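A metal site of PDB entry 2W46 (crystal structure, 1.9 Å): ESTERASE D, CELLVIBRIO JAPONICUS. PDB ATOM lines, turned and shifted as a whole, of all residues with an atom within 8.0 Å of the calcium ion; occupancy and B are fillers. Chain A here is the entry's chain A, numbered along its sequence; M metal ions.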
ATOM      1  N   LEU A   8       7.812 -32.010  -6.058  1.00  0.00           N
ATOM      2  CA  LEU A   8       8.987 -31.402  -6.678  1.00  0.00           C
ATOM      3  C   LEU A   8       9.483 -32.322  -7.770  1.00  0.00           C
ATOM      4  O   LEU A   8       9.927 -33.445  -7.497  1.00  0.00           O
ATOM      5  CB  LEU A   8      10.102 -31.141  -5.654  1.00  0.00           C
ATOM      6  CG  LEU A   8      11.379 -30.485  -6.238  1.00  0.00           C
ATOM      7  CD1 LEU A   8      11.071 -29.190  -7.042  1.00  0.00           C
ATOM      8  CD2 LEU A   8      12.381 -30.222  -5.115  1.00  0.00           C
ATOM      9  N   LEU A   9       9.339 -31.892  -9.019  1.00  0.00           N
ATOM     10  CA  LEU A   9       9.652 -32.795 -10.145  1.00  0.00           C
ATOM     11  C   LEU A   9      11.014 -32.426 -10.701  1.00  0.00           C
ATOM     12  O   LEU A   9      11.225 -31.283 -11.150  1.00  0.00           O
ATOM     13  CB  LEU A   9       8.582 -32.746 -11.240  1.00  0.00           C
ATOM     14  CG  LEU A   9       7.162 -33.126 -10.740  1.00  0.00           C
ATOM     15  CD1 LEU A   9       6.205 -32.914 -11.871  1.00  0.00           C
ATOM     16  CD2 LEU A   9       7.061 -34.586 -10.284  1.00  0.00           C
ATOM     17  N   GLN A  10      11.889 -33.431 -10.711  1.00  0.00           N
ATOM     18  CA  GLN A  10      13.252 -33.280 -11.209  1.00  0.00           C
ATOM     19  C   GLN A  10      13.383 -34.115 -12.504  1.00  0.00           C
ATOM     20  O   GLN A  10      12.655 -35.118 -12.680  1.00  0.00           O
ATOM     21  CB  GLN A  10      14.251 -33.780 -10.120  1.00  0.00           C
ATOM     22  CG  GLN A  10      14.293 -32.978  -8.806  1.00  0.00           C
ATOM     23  CD  GLN A  10      15.010 -31.626  -8.959  1.00  0.00           C
ATOM     24  OE1 GLN A  10      15.481 -31.308 -10.048  1.00  0.00           O
ATOM     25  NE2 GLN A  10      15.134 -30.863  -7.865  1.00  0.00           N
ATOM     26  N   GLU A  11      14.310 -33.738 -13.391  1.00  0.00           N
ATOM     27  CA  GLU A  11      14.871 -34.669 -14.388  1.00  0.00           C
ATOM     28  C   GLU A  11      15.212 -36.029 -13.772  1.00  0.00           C
ATOM     29  O   GLU A  11      15.634 -36.143 -12.609  1.00  0.00           O
ATOM     30  CB  GLU A  11      16.118 -34.065 -15.062  1.00  0.00           C
ATOM     31  CG  GLU A  11      17.347 -33.894 -14.098  1.00  0.00           C
ATOM     32  CD  GLU A  11      17.137 -32.790 -13.080  1.00  0.00           C
ATOM     33  OE1 GLU A  11      16.395 -31.810 -13.401  1.00  0.00           O
ATOM     34  OE2 GLU A  11      17.745 -32.809 -11.962  1.00  0.00           O
ATOM     35  N   ALA A  12      15.015 -37.079 -14.556  1.00  0.00           N
ATOM     36  CA  ALA A  12      15.394 -38.422 -14.147  1.00  0.00           C
ATOM     37  C   ALA A  12      14.637 -38.972 -12.956  1.00  0.00           C
ATOM     38  O   ALA A  12      15.153 -39.865 -12.251  1.00  0.00           O
ATOM     39  CB  ALA A  12      16.918 -38.523 -13.914  1.00  0.00           C
ATOM     40  N   PHE A  16       8.776 -36.824 -14.804  1.00  0.00           N
ATOM     41  CA  PHE A  16       9.497 -36.045 -15.807  1.00  0.00           C
ATOM     42  C   PHE A  16       9.380 -36.810 -17.115  1.00  0.00           C
ATOM     43  O   PHE A  16       9.786 -37.968 -17.195  1.00  0.00           O
ATOM     44  CB  PHE A  16      10.972 -35.842 -15.427  1.00  0.00           C
ATOM     45  CG  PHE A  16      11.726 -34.935 -16.393  1.00  0.00           C
ATOM     46  CD1 PHE A  16      11.871 -33.565 -16.119  1.00  0.00           C
ATOM     47  CD2 PHE A  16      12.266 -35.444 -17.564  1.00  0.00           C
ATOM     48  CE1 PHE A  16      12.589 -32.719 -17.024  1.00  0.00           C
ATOM     49  CE2 PHE A  16      12.956 -34.596 -18.487  1.00  0.00           C
ATOM     50  CZ  PHE A  16      13.107 -33.231 -18.190  1.00  0.00           C
ATOM     51  N   ILE A  23      19.591 -33.297 -20.936  1.00  0.00           N
ATOM     52  CA  ILE A  23      19.719 -33.078 -19.496  1.00  0.00           C
ATOM     53  C   ILE A  23      21.213 -32.878 -19.221  1.00  0.00           C
ATOM     54  O   ILE A  23      22.016 -33.776 -19.500  1.00  0.00           O
ATOM     55  CB  ILE A  23      19.176 -34.240 -18.663  1.00  0.00           C
ATOM     56  CG1 ILE A  23      17.699 -34.504 -18.970  1.00  0.00           C
ATOM     57  CG2 ILE A  23      19.391 -34.005 -17.112  1.00  0.00           C
ATOM     58  CD1 ILE A  23      16.799 -33.323 -18.670  1.00  0.00           C
ATOM     59  N   ASP A  24      21.563 -31.721 -18.683  1.00  0.00           N
ATOM     60  CA  ASP A  24      22.953 -31.273 -18.527  1.00  0.00           C
ATOM     61  C   ASP A  24      23.218 -30.998 -17.055  1.00  0.00           C
ATOM     62  O   ASP A  24      22.293 -30.979 -16.221  1.00  0.00           O
ATOM     63  CB  ASP A  24      23.235 -29.982 -19.304  1.00  0.00           C
ATOM     64  CG  ASP A  24      23.218 -30.178 -20.812  1.00  0.00           C
ATOM     65  OD1 ASP A  24      22.943 -31.292 -21.252  1.00  0.00           O
ATOM     66  OD2 ASP A  24      23.489 -29.181 -21.536  1.00  0.00           O
ATOM     67  N   GLY A  29      24.691 -24.979  -9.284  1.00  0.00           N
ATOM     68  CA  GLY A  29      23.494 -24.398  -8.647  1.00  0.00           C
ATOM     69  C   GLY A  29      22.154 -25.049  -8.906  1.00  0.00           C
ATOM     70  O   GLY A  29      21.125 -24.613  -8.365  1.00  0.00           O
ATOM     71  N   PHE A  30      22.128 -26.100  -9.732  1.00  0.00           N
ATOM     72  CA  PHE A  30      20.897 -26.858  -9.963  1.00  0.00           C
ATOM     73  C   PHE A  30      20.590 -27.752  -8.747  1.00  0.00           C
ATOM     74  O   PHE A  30      21.405 -27.829  -7.810  1.00  0.00           O
ATOM     75  CB  PHE A  30      21.029 -27.699 -11.243  1.00  0.00           C
ATOM     76  CG  PHE A  30      22.198 -28.698 -11.223  1.00  0.00           C
ATOM     77  CD1 PHE A  30      22.039 -29.987 -10.661  1.00  0.00           C
ATOM     78  CD2 PHE A  30      23.429 -28.359 -11.785  1.00  0.00           C
ATOM     79  CE1 PHE A  30      23.097 -30.877 -10.656  1.00  0.00           C
ATOM     80  CE2 PHE A  30      24.501 -29.262 -11.813  1.00  0.00           C
ATOM     81  CZ  PHE A  30      24.340 -30.525 -11.218  1.00  0.00           C
ATOM     82  N   THR A  31      19.439 -28.431  -8.791  1.00  0.00           N
ATOM     83  CA  THR A  31      19.061 -29.413  -7.766  1.00  0.00           C
ATOM     84  C   THR A  31      18.757 -30.731  -8.470  1.00  0.00           C
ATOM     85  O   THR A  31      18.566 -30.741  -9.680  1.00  0.00           O
ATOM     86  CB  THR A  31      17.842 -28.954  -6.899  1.00  0.00           C
ATOM     87  OG1 THR A  31      16.733 -28.625  -7.742  1.00  0.00           O
ATOM     88  CG2 THR A  31      18.184 -27.685  -6.104  1.00  0.00           C
ATOM     89  N   GLY A  32      18.719 -31.854  -7.741  1.00  0.00           N
ATOM     90  CA  GLY A  32      18.619 -33.147  -8.430  1.00  0.00           C
ATOM     91  C   GLY A  32      19.917 -33.456  -9.184  1.00  0.00           C
ATOM     92  O   GLY A  32      20.980 -32.988  -8.792  1.00  0.00           O
ATOM     93  N   SER A  33      19.834 -34.249 -10.260  1.00  0.00           N
ATOM     94  CA  SER A  33      21.041 -34.647 -10.993  1.00  0.00           C
ATOM     95  C   SER A  33      21.376 -33.699 -12.170  1.00  0.00           C
ATOM     96  O   SER A  33      22.425 -33.834 -12.800  1.00  0.00           O
ATOM     97  CB  SER A  33      20.908 -36.086 -11.515  1.00  0.00           C
ATOM     98  OG  SER A  33      19.709 -36.242 -12.297  1.00  0.00           O
ATOM     99  N   GLY A  34      20.500 -32.745 -12.469  1.00  0.00           N
ATOM    100  CA  GLY A  34      20.781 -31.864 -13.608  1.00  0.00           C
ATOM    101  C   GLY A  34      19.769 -30.762 -13.837  1.00  0.00           C
ATOM    102  O   GLY A  34      19.164 -30.252 -12.891  1.00  0.00           O
ATOM    103  N   PHE A  35      19.657 -30.369 -15.098  1.00  0.00           N
ATOM    104  CA  PHE A  35      18.634 -29.417 -15.532  1.00  0.00           C
ATOM    105  C   PHE A  35      18.368 -29.721 -16.993  1.00  0.00           C
ATOM    106  O   PHE A  35      19.233 -30.292 -17.703  1.00  0.00           O
ATOM    107  CB  PHE A  35      19.124 -27.956 -15.347  1.00  0.00           C
ATOM    108  CG  PHE A  35      20.529 -27.672 -15.908  1.00  0.00           C
ATOM    109  CD1 PHE A  35      20.728 -27.353 -17.270  1.00  0.00           C
ATOM    110  CD2 PHE A  35      21.642 -27.702 -15.076  1.00  0.00           C
ATOM    111  CE1 PHE A  35      22.057 -27.086 -17.766  1.00  0.00           C
ATOM    112  CE2 PHE A  35      22.910 -27.434 -15.552  1.00  0.00           C
ATOM    113  CZ  PHE A  35      23.120 -27.140 -16.888  1.00  0.00           C
ATOM    114  N   ALA A  36      17.201 -29.325 -17.471  1.00  0.00           N
ATOM    115  CA  ALA A  36      16.882 -29.480 -18.901  1.00  0.00           C
ATOM    116  C   ALA A  36      17.414 -28.291 -19.682  1.00  0.00           C
ATOM    117  O   ALA A  36      17.168 -27.134 -19.308  1.00  0.00           O
ATOM    118  CB  ALA A  36      15.385 -29.613 -19.078  1.00  0.00           C
ATOM    119  N   ARG A  63      11.985 -23.385 -11.478  1.00  0.00           N
ATOM    120  CA  ARG A  63      13.290 -22.833 -11.146  1.00  0.00           C
ATOM    121  C   ARG A  63      14.137 -22.898 -12.415  1.00  0.00           C
ATOM    122  O   ARG A  63      14.176 -23.935 -13.113  1.00  0.00           O
ATOM    123  CB  ARG A  63      13.916 -23.657 -10.026  1.00  0.00           C
ATOM    124  CG  ARG A  63      15.217 -23.082  -9.488  1.00  0.00           C
ATOM    125  CD  ARG A  63      15.569 -23.690  -8.080  1.00  0.00           C
ATOM    126  NE  ARG A  63      16.754 -23.041  -7.503  1.00  0.00           N
ATOM    127  CZ  ARG A  63      18.016 -23.426  -7.719  1.00  0.00           C
ATOM    128  NH1 ARG A  63      18.292 -24.492  -8.461  1.00  0.00           N
ATOM    129  NH2 ARG A  63      19.029 -22.745  -7.161  1.00  0.00           N
ATOM    130  N   TRP A  99      20.126 -18.962 -10.511  1.00  0.00           N
ATOM    131  CA  TRP A  99      18.831 -19.591 -10.760  1.00  0.00           C
ATOM    132  C   TRP A  99      17.805 -18.719 -10.090  1.00  0.00           C
ATOM    133  O   TRP A  99      18.073 -18.143  -9.060  1.00  0.00           O
ATOM    134  CB  TRP A  99      18.778 -21.015 -10.145  1.00  0.00           C
ATOM    135  CG  TRP A  99      19.817 -21.889 -10.720  1.00  0.00           C
ATOM    136  CD1 TRP A  99      21.153 -21.911 -10.392  1.00  0.00           C
ATOM    137  CD2 TRP A  99      19.659 -22.817 -11.824  1.00  0.00           C
ATOM    138  NE1 TRP A  99      21.825 -22.799 -11.200  1.00  0.00           N
ATOM    139  CE2 TRP A  99      20.942 -23.369 -12.080  1.00  0.00           C
ATOM    140  CE3 TRP A  99      18.577 -23.219 -12.616  1.00  0.00           C
ATOM    141  CZ2 TRP A  99      21.161 -24.325 -13.088  1.00  0.00           C
ATOM    142  CZ3 TRP A  99      18.791 -24.187 -13.630  1.00  0.00           C
ATOM    143  CH2 TRP A  99      20.076 -24.733 -13.851  1.00  0.00           C
ATOM    144  N   ILE A 128      16.134 -25.391 -17.346  1.00  0.00           N
ATOM    145  CA  ILE A 128      15.032 -25.600 -16.404  1.00  0.00           C
ATOM    146  C   ILE A 128      15.445 -26.637 -15.362  1.00  0.00           C
ATOM    147  O   ILE A 128      15.688 -27.798 -15.693  1.00  0.00           O
ATOM    148  CB  ILE A 128      13.723 -26.100 -17.118  1.00  0.00           C
ATOM    149  CG1 ILE A 128      13.237 -25.147 -18.258  1.00  0.00           C
ATOM    150  CG2 ILE A 128      12.656 -26.370 -16.091  1.00  0.00           C
ATOM    151  CD1 ILE A 128      12.955 -23.731 -17.837  1.00  0.00           C
ATOM    152  N   ASP A 129      15.590 -26.186 -14.116  1.00  0.00           N
ATOM    153  CA  ASP A 129      16.065 -27.068 -13.030  1.00  0.00           C
ATOM    154  C   ASP A 129      14.965 -28.018 -12.513  1.00  0.00           C
ATOM    155  O   ASP A 129      15.201 -29.219 -12.314  1.00  0.00           O
ATOM    156  CB  ASP A 129      16.560 -26.203 -11.866  1.00  0.00           C
ATOM    157  CG  ASP A 129      17.079 -27.037 -10.672  1.00  0.00           C
ATOM    158  OD1 ASP A 129      17.691 -28.111 -10.887  1.00  0.00           O
ATOM    159  OD2 ASP A 129      16.928 -26.585  -9.537  1.00  0.00           O
ATOM    160  N   SER A 130      13.772 -27.477 -12.258  1.00  0.00           N
ATOM    161  CA  SER A 130      12.735 -28.264 -11.582  1.00  0.00           C
ATOM    162  C   SER A 130      11.356 -27.591 -11.737  1.00  0.00           C
ATOM    163  O   SER A 130      11.261 -26.396 -12.096  1.00  0.00           O
ATOM    164  CB  SER A 130      13.083 -28.383 -10.097  1.00  0.00           C
ATOM    165  OG  SER A 130      13.174 -27.091  -9.467  1.00  0.00           O
ATOM    166  N   LEU A 131      10.299 -28.391 -11.500  1.00  0.00           N
ATOM    167  CA  LEU A 131       8.931 -27.880 -11.387  1.00  0.00           C
ATOM    168  C   LEU A 131       8.403 -28.267 -10.008  1.00  0.00           C
ATOM    169  O   LEU A 131       8.470 -29.444  -9.633  1.00  0.00           O
ATOM    170  CB  LEU A 131       8.011 -28.489 -12.460  1.00  0.00           C
ATOM    171  CG  LEU A 131       6.534 -28.098 -12.367  1.00  0.00           C
ATOM    172  CD1 LEU A 131       6.358 -26.610 -12.668  1.00  0.00           C
ATOM    173  CD2 LEU A 131       5.700 -28.948 -13.375  1.00  0.00           C
HETATM  174 CA    CA M   1      17.112 -30.457 -11.497  1.00  0.00          CA
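Within 4 Å of the calcium ion: Gln 10, Glu 11, Thr 31, Gly 34 and Asp 129.
The nearest printed residue that does not touch the calcium ion is Gly 32 (4.3 Å).
The side-chain amide oxygen (OE1) of Gln 10 is bound to the calcium ion, 2.3 Å away.
O of Thr 31 binds the calcium ion (2.3 Å).
O of Asp 129 is bound to the calcium ion (2.4 Å).
OE1 of Glu 11 binds the calcium ion, at 2.4 Å.
The side-chain carboxylate (OE2) of Glu 11 is bound to the calcium ion, at 2.5 Å.
The calcium ion is bound by O of Gly 34, at 2.5 Å.
OD1 of Asp 129 is bound to the calcium ion, 2.5 Å away.
The side-chain carboxylate (OD2) of Asp 129 lies within salt-bridge range of the guanidinium group (NH1) of Arg 63, 2.7 Å away.
The side-chain carboxylate (OE2) of Glu 11 lies close to the backbone NH (N) of Ser 33, at 3.1 Å.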
